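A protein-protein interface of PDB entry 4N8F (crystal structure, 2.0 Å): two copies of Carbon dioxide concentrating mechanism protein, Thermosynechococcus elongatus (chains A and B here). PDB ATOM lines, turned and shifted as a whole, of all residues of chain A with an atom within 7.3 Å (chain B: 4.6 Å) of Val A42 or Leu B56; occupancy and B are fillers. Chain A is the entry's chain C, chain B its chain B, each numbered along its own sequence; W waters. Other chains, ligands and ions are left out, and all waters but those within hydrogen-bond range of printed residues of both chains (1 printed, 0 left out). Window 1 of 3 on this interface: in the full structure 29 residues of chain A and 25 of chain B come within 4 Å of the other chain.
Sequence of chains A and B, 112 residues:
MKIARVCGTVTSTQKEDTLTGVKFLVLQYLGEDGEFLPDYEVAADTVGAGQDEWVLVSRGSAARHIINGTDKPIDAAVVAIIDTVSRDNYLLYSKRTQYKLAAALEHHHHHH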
ATOM      1  N   THR A   9      -3.651 -24.713 -26.204  1.00  0.00           N
ATOM      2  CA  THR A   9      -4.106 -23.649 -25.357  1.00  0.00           C
ATOM      3  C   THR A   9      -4.518 -22.439 -26.199  1.00  0.00           C
ATOM      4  O   THR A   9      -4.046 -22.271 -27.340  1.00  0.00           O
ATOM      5  CB  THR A   9      -2.980 -23.109 -24.456  1.00  0.00           C
ATOM      6  OG1 THR A   9      -2.024 -22.491 -25.293  1.00  0.00           O
ATOM      7  CG2 THR A   9      -2.292 -24.185 -23.725  1.00  0.00           C
ATOM      8  N   VAL A  10      -5.376 -21.598 -25.614  1.00  0.00           N
ATOM      9  CA  VAL A  10      -5.745 -20.273 -26.188  1.00  0.00           C
ATOM     10  C   VAL A  10      -5.357 -19.162 -25.208  1.00  0.00           C
ATOM     11  O   VAL A  10      -5.562 -19.254 -23.963  1.00  0.00           O
ATOM     12  CB  VAL A  10      -7.274 -20.218 -26.431  1.00  0.00           C
ATOM     13  CG1 VAL A  10      -7.744 -18.828 -26.885  1.00  0.00           C
ATOM     14  CG2 VAL A  10      -7.711 -21.316 -27.402  1.00  0.00           C
ATOM     15  N   THR A  11      -4.802 -18.094 -25.748  1.00  0.00           N
ATOM     16  CA  THR A  11      -4.494 -16.919 -24.906  1.00  0.00           C
ATOM     17  C   THR A  11      -5.271 -15.706 -25.417  1.00  0.00           C
ATOM     18  O   THR A  11      -5.547 -15.592 -26.640  1.00  0.00           O
ATOM     19  CB  THR A  11      -2.987 -16.601 -24.920  1.00  0.00           C
ATOM     20  OG1 THR A  11      -2.668 -16.086 -26.204  1.00  0.00           O
ATOM     21  CG2 THR A  11      -2.152 -17.862 -24.648  1.00  0.00           C
ATOM     22  N   SER A  12      -5.650 -14.824 -24.483  1.00  0.00           N
ATOM     23  CA  SER A  12      -6.426 -13.628 -24.803  1.00  0.00           C
ATOM     24  C   SER A  12      -6.053 -12.538 -23.835  1.00  0.00           C
ATOM     25  O   SER A  12      -6.023 -12.778 -22.652  1.00  0.00           O
ATOM     26  CB  SER A  12      -7.903 -13.911 -24.629  1.00  0.00           C
ATOM     27  OG  SER A  12      -8.666 -12.735 -24.711  1.00  0.00           O
ATOM     28  N   LYS A  15     -10.804  -9.378 -22.963  1.00  0.00           N
ATOM     29  CA  LYS A  15     -11.772 -10.417 -22.526  1.00  0.00           C
ATOM     30  C   LYS A  15     -12.583  -9.882 -21.352  1.00  0.00           C
ATOM     31  O   LYS A  15     -12.165  -8.917 -20.716  1.00  0.00           O
ATOM     32  CB  LYS A  15     -11.055 -11.728 -22.156  1.00  0.00           C
ATOM     33  CG  LYS A  15     -10.075 -11.589 -20.990  1.00  0.00           C
ATOM     34  CD  LYS A  15      -9.193 -12.825 -20.785  1.00  0.00           C
ATOM     35  CE  LYS A  15      -7.990 -12.445 -19.936  1.00  0.00           C
ATOM     36  NZ  LYS A  15      -6.838 -13.336 -20.194  1.00  0.00           N
ATOM     37  N   LEU A  19     -12.959 -13.260 -16.526  1.00  0.00           N
ATOM     38  CA  LEU A  19     -12.035 -14.262 -17.002  1.00  0.00           C
ATOM     39  C   LEU A  19     -10.559 -13.997 -16.755  1.00  0.00           C
ATOM     40  O   LEU A  19      -9.748 -14.770 -17.211  1.00  0.00           O
ATOM     41  CB  LEU A  19     -12.246 -14.504 -18.486  1.00  0.00           C
ATOM     42  CG  LEU A  19     -13.680 -14.830 -18.850  1.00  0.00           C
ATOM     43  CD1 LEU A  19     -13.779 -15.052 -20.346  1.00  0.00           C
ATOM     44  CD2 LEU A  19     -14.097 -16.047 -18.051  1.00  0.00           C
ATOM     45  N   LYS A  23      -7.149 -20.097 -17.203  1.00  0.00           N
ATOM     46  CA  LYS A  23      -6.491 -20.885 -18.213  1.00  0.00           C
ATOM     47  C   LYS A  23      -7.448 -21.518 -19.212  1.00  0.00           C
ATOM     48  O   LYS A  23      -8.357 -22.246 -18.840  1.00  0.00           O
ATOM     49  CB  LYS A  23      -5.590 -21.958 -17.596  1.00  0.00           C
ATOM     50  CG  LYS A  23      -4.404 -22.240 -18.526  1.00  0.00           C
ATOM     51  CD  LYS A  23      -3.847 -23.645 -18.371  1.00  0.00           C
ATOM     52  CE  LYS A  23      -2.887 -23.971 -19.513  1.00  0.00           C
ATOM     53  NZ  LYS A  23      -1.900 -22.910 -19.772  1.00  0.00           N
ATOM     54  N   PHE A  24      -7.241 -21.248 -20.484  1.00  0.00           N
ATOM     55  CA  PHE A  24      -8.015 -21.864 -21.572  1.00  0.00           C
ATOM     56  C   PHE A  24      -7.275 -22.993 -22.321  1.00  0.00           C
ATOM     57  O   PHE A  24      -6.326 -22.767 -23.085  1.00  0.00           O
ATOM     58  CB  PHE A  24      -8.440 -20.824 -22.606  1.00  0.00           C
ATOM     59  CG  PHE A  24      -9.221 -19.670 -22.035  1.00  0.00           C
ATOM     60  CD1 PHE A  24     -10.477 -19.840 -21.603  1.00  0.00           C
ATOM     61  CD2 PHE A  24      -8.662 -18.410 -21.940  1.00  0.00           C
ATOM     62  CE1 PHE A  24     -11.204 -18.788 -21.105  1.00  0.00           C
ATOM     63  CE2 PHE A  24      -9.383 -17.346 -21.433  1.00  0.00           C
ATOM     64  CZ  PHE A  24     -10.663 -17.536 -21.034  1.00  0.00           C
ATOM     65  N   LEU A  25      -7.768 -24.218 -22.166  1.00  0.00           N
ATOM     66  CA  LEU A  25      -7.139 -25.315 -22.867  1.00  0.00           C
ATOM     67  C   LEU A  25      -7.931 -25.572 -24.100  1.00  0.00           C
ATOM     68  O   LEU A  25      -9.128 -25.413 -24.082  1.00  0.00           O
ATOM     69  CB  LEU A  25      -7.098 -26.558 -21.972  1.00  0.00           C
ATOM     70  CG  LEU A  25      -6.171 -26.544 -20.757  1.00  0.00           C
ATOM     71  CD1 LEU A  25      -6.310 -27.875 -20.035  1.00  0.00           C
ATOM     72  CD2 LEU A  25      -4.722 -26.312 -21.135  1.00  0.00           C
ATOM     73  N   VAL A  26      -7.258 -25.983 -25.174  1.00  0.00           N
ATOM     74  CA  VAL A  26      -7.927 -26.642 -26.271  1.00  0.00           C
ATOM     75  C   VAL A  26      -8.012 -28.162 -26.041  1.00  0.00           C
ATOM     76  O   VAL A  26      -7.020 -28.799 -25.717  1.00  0.00           O
ATOM     77  CB  VAL A  26      -7.211 -26.364 -27.581  1.00  0.00           C
ATOM     78  CG1 VAL A  26      -8.015 -26.908 -28.746  1.00  0.00           C
ATOM     79  CG2 VAL A  26      -6.928 -24.875 -27.741  1.00  0.00           C
ATOM     80  N   LEU A  27      -9.196 -28.732 -26.200  1.00  0.00           N
ATOM     81  CA  LEU A  27      -9.487 -30.161 -26.008  1.00  0.00           C
ATOM     82  C   LEU A  27      -9.933 -30.786 -27.355  1.00  0.00           C
ATOM     83  O   LEU A  27     -10.717 -30.192 -28.094  1.00  0.00           O
ATOM     84  CB  LEU A  27     -10.606 -30.314 -24.999  1.00  0.00           C
ATOM     85  CG  LEU A  27     -10.419 -29.601 -23.644  1.00  0.00           C
ATOM     86  CD1 LEU A  27     -11.483 -29.940 -22.622  1.00  0.00           C
ATOM     87  CD2 LEU A  27      -9.088 -29.994 -23.022  1.00  0.00           C
ATOM     88  N   TYR A  29     -11.942 -33.970 -28.632  1.00  0.00           N
ATOM     89  CA  TYR A  29     -12.790 -35.050 -28.179  1.00  0.00           C
ATOM     90  C   TYR A  29     -12.260 -36.419 -28.609  1.00  0.00           C
ATOM     91  O   TYR A  29     -11.726 -36.545 -29.696  1.00  0.00           O
ATOM     92  CB  TYR A  29     -14.265 -34.836 -28.642  1.00  0.00           C
ATOM     93  CG  TYR A  29     -14.959 -33.684 -27.926  1.00  0.00           C
ATOM     94  CD1 TYR A  29     -15.218 -32.499 -28.575  1.00  0.00           C
ATOM     95  CD2 TYR A  29     -15.330 -33.794 -26.572  1.00  0.00           C
ATOM     96  CE1 TYR A  29     -15.850 -31.466 -27.943  1.00  0.00           C
ATOM     97  CE2 TYR A  29     -15.972 -32.781 -25.940  1.00  0.00           C
ATOM     98  CZ  TYR A  29     -16.203 -31.598 -26.598  1.00  0.00           C
ATOM     99  OH  TYR A  29     -16.808 -30.545 -25.941  1.00  0.00           O
ATOM    100  N   TYR A  40     -13.623 -30.262 -31.265  1.00  0.00           N
ATOM    101  CA  TYR A  40     -12.747 -29.586 -30.291  1.00  0.00           C
ATOM    102  C   TYR A  40     -13.591 -28.688 -29.349  1.00  0.00           C
ATOM    103  O   TYR A  40     -14.705 -28.339 -29.669  1.00  0.00           O
ATOM    104  CB  TYR A  40     -11.657 -28.744 -31.013  1.00  0.00           C
ATOM    105  CG  TYR A  40     -12.248 -27.436 -31.422  1.00  0.00           C
ATOM    106  CD1 TYR A  40     -12.887 -27.307 -32.641  1.00  0.00           C
ATOM    107  CD2 TYR A  40     -12.282 -26.357 -30.523  1.00  0.00           C
ATOM    108  CE1 TYR A  40     -13.499 -26.128 -32.993  1.00  0.00           C
ATOM    109  CE2 TYR A  40     -12.912 -25.167 -30.859  1.00  0.00           C
ATOM    110  CZ  TYR A  40     -13.517 -25.061 -32.093  1.00  0.00           C
ATOM    111  OH  TYR A  40     -14.149 -23.902 -32.445  1.00  0.00           O
ATOM    112  N   GLU A  41     -13.079 -28.407 -28.156  1.00  0.00           N
ATOM    113  CA  GLU A  41     -13.709 -27.479 -27.218  1.00  0.00           C
ATOM    114  C   GLU A  41     -12.629 -26.594 -26.635  1.00  0.00           C
ATOM    115  O   GLU A  41     -11.525 -27.045 -26.416  1.00  0.00           O
ATOM    116  CB  GLU A  41     -14.359 -28.269 -26.074  1.00  0.00           C
ATOM    117  CG  GLU A  41     -15.396 -27.498 -25.270  1.00  0.00           C
ATOM    118  CD  GLU A  41     -16.681 -27.138 -26.013  1.00  0.00           C
ATOM    119  OE1 GLU A  41     -17.207 -26.025 -25.739  1.00  0.00           O
ATOM    120  OE2 GLU A  41     -17.147 -27.924 -26.837  1.00  0.00           O
ATOM    121  N   VAL A  42     -12.917 -25.353 -26.352  1.00  0.00           N
ATOM    122  CA  VAL A  42     -11.983 -24.609 -25.517  1.00  0.00           C
ATOM    123  C   VAL A  42     -12.583 -24.542 -24.137  1.00  0.00           C
ATOM    124  O   VAL A  42     -13.776 -24.236 -23.983  1.00  0.00           O
ATOM    125  CB  VAL A  42     -11.734 -23.190 -26.058  1.00  0.00           C
ATOM    126  CG1 VAL A  42     -10.819 -22.399 -25.109  1.00  0.00           C
ATOM    127  CG2 VAL A  42     -11.175 -23.260 -27.453  1.00  0.00           C
ATOM    128  N   ALA A  43     -11.804 -24.922 -23.134  1.00  0.00           N
ATOM    129  CA  ALA A  43     -12.328 -25.059 -21.805  1.00  0.00           C
ATOM    130  C   ALA A  43     -11.454 -24.445 -20.754  1.00  0.00           C
ATOM    131  O   ALA A  43     -10.250 -24.519 -20.827  1.00  0.00           O
ATOM    132  CB  ALA A  43     -12.516 -26.517 -21.497  1.00  0.00           C
ATOM    133  N   ALA A  44     -12.102 -23.903 -19.736  1.00  0.00           N
ATOM    134  CA  ALA A  44     -11.433 -23.472 -18.487  1.00  0.00           C
ATOM    135  C   ALA A  44     -10.877 -24.638 -17.744  1.00  0.00           C
ATOM    136  O   ALA A  44     -11.436 -25.774 -17.776  1.00  0.00           O
ATOM    137  CB  ALA A  44     -12.389 -22.703 -17.563  1.00  0.00           C
ATOM    138  N   VAL A  57     -14.685 -33.312 -19.577  1.00  0.00           N
ATOM    139  CA  VAL A  57     -15.173 -31.969 -19.718  1.00  0.00           C
ATOM    140  C   VAL A  57     -16.687 -31.897 -19.467  1.00  0.00           C
ATOM    141  O   VAL A  57     -17.444 -32.760 -19.898  1.00  0.00           O
ATOM    142  CB  VAL A  57     -14.702 -31.346 -21.067  1.00  0.00           C
ATOM    143  CG1 VAL A  57     -15.066 -32.184 -22.230  1.00  0.00           C
ATOM    144  CG2 VAL A  57     -15.334 -29.987 -21.290  1.00  0.00           C
ATOM    145  N   ILE A  74     -18.554 -18.863 -18.835  1.00  0.00           N
ATOM    146  CA  ILE A  74     -17.932 -20.049 -19.449  1.00  0.00           C
ATOM    147  C   ILE A  74     -18.946 -21.159 -19.525  1.00  0.00           C
ATOM    148  O   ILE A  74     -19.803 -21.301 -18.615  1.00  0.00           O
ATOM    149  CB  ILE A  74     -16.679 -20.523 -18.695  1.00  0.00           C
ATOM    150  CG1 ILE A  74     -16.979 -20.655 -17.191  1.00  0.00           C
ATOM    151  CG2 ILE A  74     -15.551 -19.526 -18.841  1.00  0.00           C
ATOM    152  CD1 ILE A  74     -15.925 -21.483 -16.488  1.00  0.00           C
ATOM    153  N   ASP A  75     -18.844 -21.939 -20.603  1.00  0.00           N
ATOM    154  CA  ASP A  75     -19.750 -23.012 -20.908  1.00  0.00           C
ATOM    155  C   ASP A  75     -19.023 -24.367 -21.086  1.00  0.00           C
ATOM    156  O   ASP A  75     -19.570 -25.315 -21.541  1.00  0.00           O
ATOM    157  CB  ASP A  75     -20.563 -22.644 -22.134  1.00  0.00           C
ATOM    158  CG  ASP A  75     -19.783 -22.630 -23.399  1.00  0.00           C
ATOM    159  OD1 ASP A  75     -18.529 -22.707 -23.370  1.00  0.00           O
ATOM    160  OD2 ASP A  75     -20.460 -22.552 -24.484  1.00  0.00           O
ATOM    161  N   ALA A  76     -17.751 -24.424 -20.748  1.00  0.00           N
ATOM    162  CA  ALA A  76     -16.976 -25.676 -20.809  1.00  0.00           C
ATOM    163  C   ALA A  76     -15.846 -25.604 -19.790  1.00  0.00           C
ATOM    164  O   ALA A  76     -15.120 -24.579 -19.712  1.00  0.00           O
ATOM    165  CB  ALA A  76     -16.421 -25.880 -22.170  1.00  0.00           C
ATOM    166  N   ALA A  77     -15.664 -26.671 -19.025  1.00  0.00           N
ATOM    167  CA  ALA A  77     -14.557 -26.712 -18.063  1.00  0.00           C
ATOM    168  C   ALA A  77     -14.005 -28.106 -17.950  1.00  0.00           C
ATOM    169  O   ALA A  77     -14.799 -29.075 -17.940  1.00  0.00           O
ATOM    170  CB  ALA A  77     -15.008 -26.270 -16.685  1.00  0.00           C
ATOM    171  N   MET B   1     -16.483 -23.618 -24.761  1.00  0.00           N
ATOM    172  CA  MET B   1     -16.390 -22.470 -25.682  1.00  0.00           C
ATOM    173  C   MET B   1     -15.909 -22.967 -27.051  1.00  0.00           C
ATOM    174  O   MET B   1     -15.290 -24.009 -27.162  1.00  0.00           O
ATOM    175  CB  MET B   1     -15.415 -21.416 -25.113  1.00  0.00           C
ATOM    176  CG  MET B   1     -16.015 -20.673 -23.923  1.00  0.00           C
ATOM    177  SD  MET B   1     -15.765 -21.563 -22.396  1.00  0.00           S
ATOM    178  CE  MET B   1     -14.043 -21.251 -22.024  1.00  0.00           C
ATOM    179  N   LYS B   2     -16.182 -22.189 -28.073  1.00  0.00           N
ATOM    180  CA  LYS B   2     -15.745 -22.526 -29.385  1.00  0.00           C
ATOM    181  C   LYS B   2     -14.991 -21.334 -29.899  1.00  0.00           C
ATOM    182  O   LYS B   2     -15.221 -20.224 -29.469  1.00  0.00           O
ATOM    183  CB  LYS B   2     -16.939 -22.744 -30.308  1.00  0.00           C
ATOM    184  CG  LYS B   2     -17.787 -23.907 -29.928  1.00  0.00           C
ATOM    185  CD  LYS B   2     -17.128 -25.211 -30.314  1.00  0.00           C
ATOM    186  CE  LYS B   2     -18.041 -26.359 -29.905  1.00  0.00           C
ATOM    187  NZ  LYS B   2     -17.353 -27.650 -29.969  1.00  0.00           N
ATOM    188  N   ILE B   3     -14.101 -21.609 -30.832  1.00  0.00           N
ATOM    189  CA  ILE B   3     -13.352 -20.571 -31.583  1.00  0.00           C
ATOM    190  C   ILE B   3     -14.155 -20.152 -32.801  1.00  0.00           C
ATOM    191  O   ILE B   3     -14.671 -21.002 -33.501  1.00  0.00           O
ATOM    192  CB  ILE B   3     -11.956 -21.093 -31.980  1.00  0.00           C
ATOM    193  CG1 ILE B   3     -11.149 -21.428 -30.720  1.00  0.00           C
ATOM    194  CG2 ILE B   3     -11.185 -20.029 -32.769  1.00  0.00           C
ATOM    195  CD1 ILE B   3      -9.906 -22.272 -30.950  1.00  0.00           C
ATOM    196  N   VAL B  55     -12.357 -14.983 -31.850  1.00  0.00           N
ATOM    197  CA  VAL B  55     -12.977 -14.879 -30.539  1.00  0.00           C
ATOM    198  C   VAL B  55     -13.340 -16.225 -29.946  1.00  0.00           C
ATOM    199  O   VAL B  55     -13.447 -17.224 -30.647  1.00  0.00           O
ATOM    200  CB  VAL B  55     -14.273 -14.042 -30.622  1.00  0.00           C
ATOM    201  CG1 VAL B  55     -13.998 -12.638 -31.154  1.00  0.00           C
ATOM    202  CG2 VAL B  55     -15.317 -14.696 -31.522  1.00  0.00           C
ATOM    203  N   LEU B  56     -13.483 -16.261 -28.630  1.00  0.00           N
ATOM    204  CA  LEU B  56     -14.137 -17.361 -27.937  1.00  0.00           C
ATOM    205  C   LEU B  56     -15.578 -16.984 -27.776  1.00  0.00           C
ATOM    206  O   LEU B  56     -15.891 -15.833 -27.356  1.00  0.00           O
ATOM    207  CB  LEU B  56     -13.543 -17.618 -26.542  1.00  0.00           C
ATOM    208  CG  LEU B  56     -12.126 -18.182 -26.474  1.00  0.00           C
ATOM    209  CD1 LEU B  56     -11.654 -18.389 -25.021  1.00  0.00           C
ATOM    210  CD2 LEU B  56     -12.069 -19.493 -27.248  1.00  0.00           C
ATOM    211  N   VAL B  57     -16.468 -17.945 -28.106  1.00  0.00           N
ATOM    212  CA  VAL B  57     -17.900 -17.763 -27.923  1.00  0.00           C
ATOM    213  C   VAL B  57     -18.409 -18.760 -26.827  1.00  0.00           C
ATOM    214  O   VAL B  57     -18.103 -19.938 -26.868  1.00  0.00           O
ATOM    215  CB  VAL B  57     -18.720 -18.126 -29.186  1.00  0.00           C
ATOM    216  CG1 VAL B  57     -20.166 -17.669 -29.037  1.00  0.00           C
ATOM    217  CG2 VAL B  57     -18.079 -17.573 -30.439  1.00  0.00           C
ATOM    218  N   SER B  58     -19.214 -18.266 -25.905  1.00  0.00           N
ATOM    219  CA  SER B  58     -19.897 -19.094 -24.922  1.00  0.00           C
ATOM    220  C   SER B  58     -21.359 -19.045 -25.226  1.00  0.00           C
ATOM    221  O   SER B  58     -21.895 -17.967 -25.565  1.00  0.00           O
ATOM    222  CB  SER B  58     -19.694 -18.561 -23.509  1.00  0.00           C
ATOM    223  OG  SER B  58     -18.372 -18.700 -23.053  1.00  0.00           O
ATOM    224  N   ALA B  77     -22.472 -15.289 -26.599  1.00  0.00           N
ATOM    225  CA  ALA B  77     -21.674 -14.089 -26.309  1.00  0.00           C
ATOM    226  C   ALA B  77     -20.221 -14.311 -26.589  1.00  0.00           C
ATOM    227  O   ALA B  77     -19.651 -15.363 -26.314  1.00  0.00           O
ATOM    228  CB  ALA B  77     -21.819 -13.639 -24.884  1.00  0.00           C
ATOM    229  N   VAL B  78     -19.625 -13.279 -27.194  1.00  0.00           N
ATOM    230  CA  VAL B  78     -18.202 -13.194 -27.306  1.00  0.00           C
ATOM    231  C   VAL B  78     -17.671 -12.945 -25.921  1.00  0.00           C
ATOM    232  O   VAL B  78     -18.164 -12.089 -25.206  1.00  0.00           O
ATOM    233  CB  VAL B  78     -17.826 -12.012 -28.190  1.00  0.00           C
ATOM    234  CG1 VAL B  78     -16.346 -11.783 -28.120  1.00  0.00           C
ATOM    235  CG2 VAL B  78     -18.281 -12.320 -29.613  1.00  0.00           C
ATOM    236  N   VAL B  79     -16.704 -13.732 -25.500  1.00  0.00           N
ATOM    237  CA  VAL B  79     -16.180 -13.541 -24.142  1.00  0.00           C
ATOM    238  C   VAL B  79     -14.731 -13.179 -24.123  1.00  0.00           C
ATOM    239  O   VAL B  79     -14.206 -12.764 -23.093  1.00  0.00           O
ATOM    240  CB  VAL B  79     -16.490 -14.740 -23.208  1.00  0.00           C
ATOM    241  CG1 VAL B  79     -17.986 -14.926 -23.086  1.00  0.00           C
ATOM    242  CG2 VAL B  79     -15.818 -16.034 -23.644  1.00  0.00           C
ATOM    243  N   ALA B  80     -14.077 -13.339 -25.261  1.00  0.00           N
ATOM    244  CA  ALA B  80     -12.664 -12.990 -25.364  1.00  0.00           C
ATOM    245  C   ALA B  80     -12.273 -12.826 -26.817  1.00  0.00           C
ATOM    246  O   ALA B  80     -12.777 -13.562 -27.683  1.00  0.00           O
ATOM    247  CB  ALA B  80     -11.810 -14.061 -24.725  1.00  0.00           C
ATOM    248  N   ILE B  82      -9.146 -13.470 -29.215  1.00  0.00           N
ATOM    249  CA  ILE B  82      -8.022 -14.393 -29.177  1.00  0.00           C
ATOM    250  C   ILE B  82      -6.732 -13.706 -29.669  1.00  0.00           C
ATOM    251  O   ILE B  82      -6.738 -12.998 -30.669  1.00  0.00           O
ATOM    252  CB  ILE B  82      -8.379 -15.633 -30.006  1.00  0.00           C
ATOM    253  CG1 ILE B  82      -9.545 -16.375 -29.312  1.00  0.00           C
ATOM    254  CG2 ILE B  82      -7.166 -16.505 -30.253  1.00  0.00           C
ATOM    255  CD1 ILE B  82     -10.027 -17.628 -30.003  1.00  0.00           C
HETATM  256  O   HOH W   1     -19.826 -22.397 -27.173  1.00  0.00           O
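The backbone NH (N) of Ile B3 sits at hydrogen-bond distance from the side-chain hydroxyl (OH) of Tyr A40. The backbone NH (N) of Met B1 lies within hydrogen-bond range of the side-chain carboxylate (OE1) of Glu A41 (2.7 Å). The backbone NH (N) of Val A42 is in hydrogen-bond range of the backbone carbonyl oxygen (O) of Met B1 (2.8 Å). The side-chain amino group of Lys B2 is in hydrogen-bond range of the backbone carbonyl oxygen of Tyr A40. The backbone NH (N) of Met B1 is in hydrogen-bond range of the side-chain carboxylate (OD1) of Asp A75. NZ of Lys B2 lies within salt-bridge range of OE2 of Glu A41 (3.2 Å).
OE2 of Glu A41 is in hydrogen-bond range of OH of Tyr A29, at 2.8 Å. The backbone NH (N) of Val A10 is in hydrogen-bond range of the backbone carbonyl oxygen (O) of Phe A24 (2.9 Å). The backbone carbonyl oxygen (O) of Leu B56 is in hydrogen-bond range of the backbone NH (N) of Val B79 (2.9 Å). The backbone NH of Ala B77 lies within hydrogen-bond range of the backbone carbonyl oxygen of Ser B58. The backbone NH (N) of Leu A27 is in hydrogen-bond range of the backbone carbonyl oxygen (O) of Glu A41 (2.9 Å). N of Leu B56 sits at hydrogen-bond distance from O of Ala B80 (2.9 Å).
Of chain B, only Met B1, Ile B3 and Leu B56 come within 4 Å of Val A42. Leu B56 touches two residues of chain A. Of the printed residues of chain B, Glu A41 touches Met B1 (2.7 Å) and Lys B2 (3.2 Å). Of the printed residues of chain A, Ile B3 touches Tyr A40 (2.8 Å) and Val A42 (3.7 Å). Of the printed residues of chain B, Val A10 touches Ile B82 (3.9 Å). Printed residues of chain B within 4 Å of Ser A12: Ala B80. The nearest printed residue of chain B that does not touch Val A42 is Lys B2 (4.9 Å).
Thr A11 touches Ile B82. Ala B80 touches Ser A12 (CB to OG, 3.4 Å). Val B79 touches Lys A15 (O to CA, 3.4 Å). Ala B80 touches Lys A15 (CB to CB, 3.6 Å). CD1 of Leu A19 touches O of Val B79 (3.6 Å). Ile B3 touches Val A42 (CG1 to CG2, 3.7 Å). CD2 of Leu B56 touches CG1 of Val A42, at 3.8 Å. Met B1 touches Ile A74 (CE to CG2, 3.9 Å). Ile A74 touches Ser B58. OD2 of Asp A75 touches CA of Ser B58, 3.5 Å away.
Positions printed for both chains: 57 and 77. Of the 20 pairs that touch across the chains among the printed residues, none has its exchanged pair printed and touching as well.
Water W1 lies within hydrogen-bond range of OD2 of Asp A75 (2.8 Å) and O of Val B57 (3.0 Å).
Hydrophobic or aromatic side chains of chain A that line the printed part of chain B: Val A10, Leu A19, Phe A24, Tyr A40, Val A42, Ile A74 and Ala A76. Printed residues of chain B that touch a printed residue of chain A: Met B1, Lys B2, Ile B3, Leu B56, Ser B58, Val B79, Ala B80 and Ile B82. Among the printed residues, Asp or Glu carboxylates within 4 Å of a Lys or Arg side-chain nitrogen of the other chain: Glu A41 with Lys B2.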
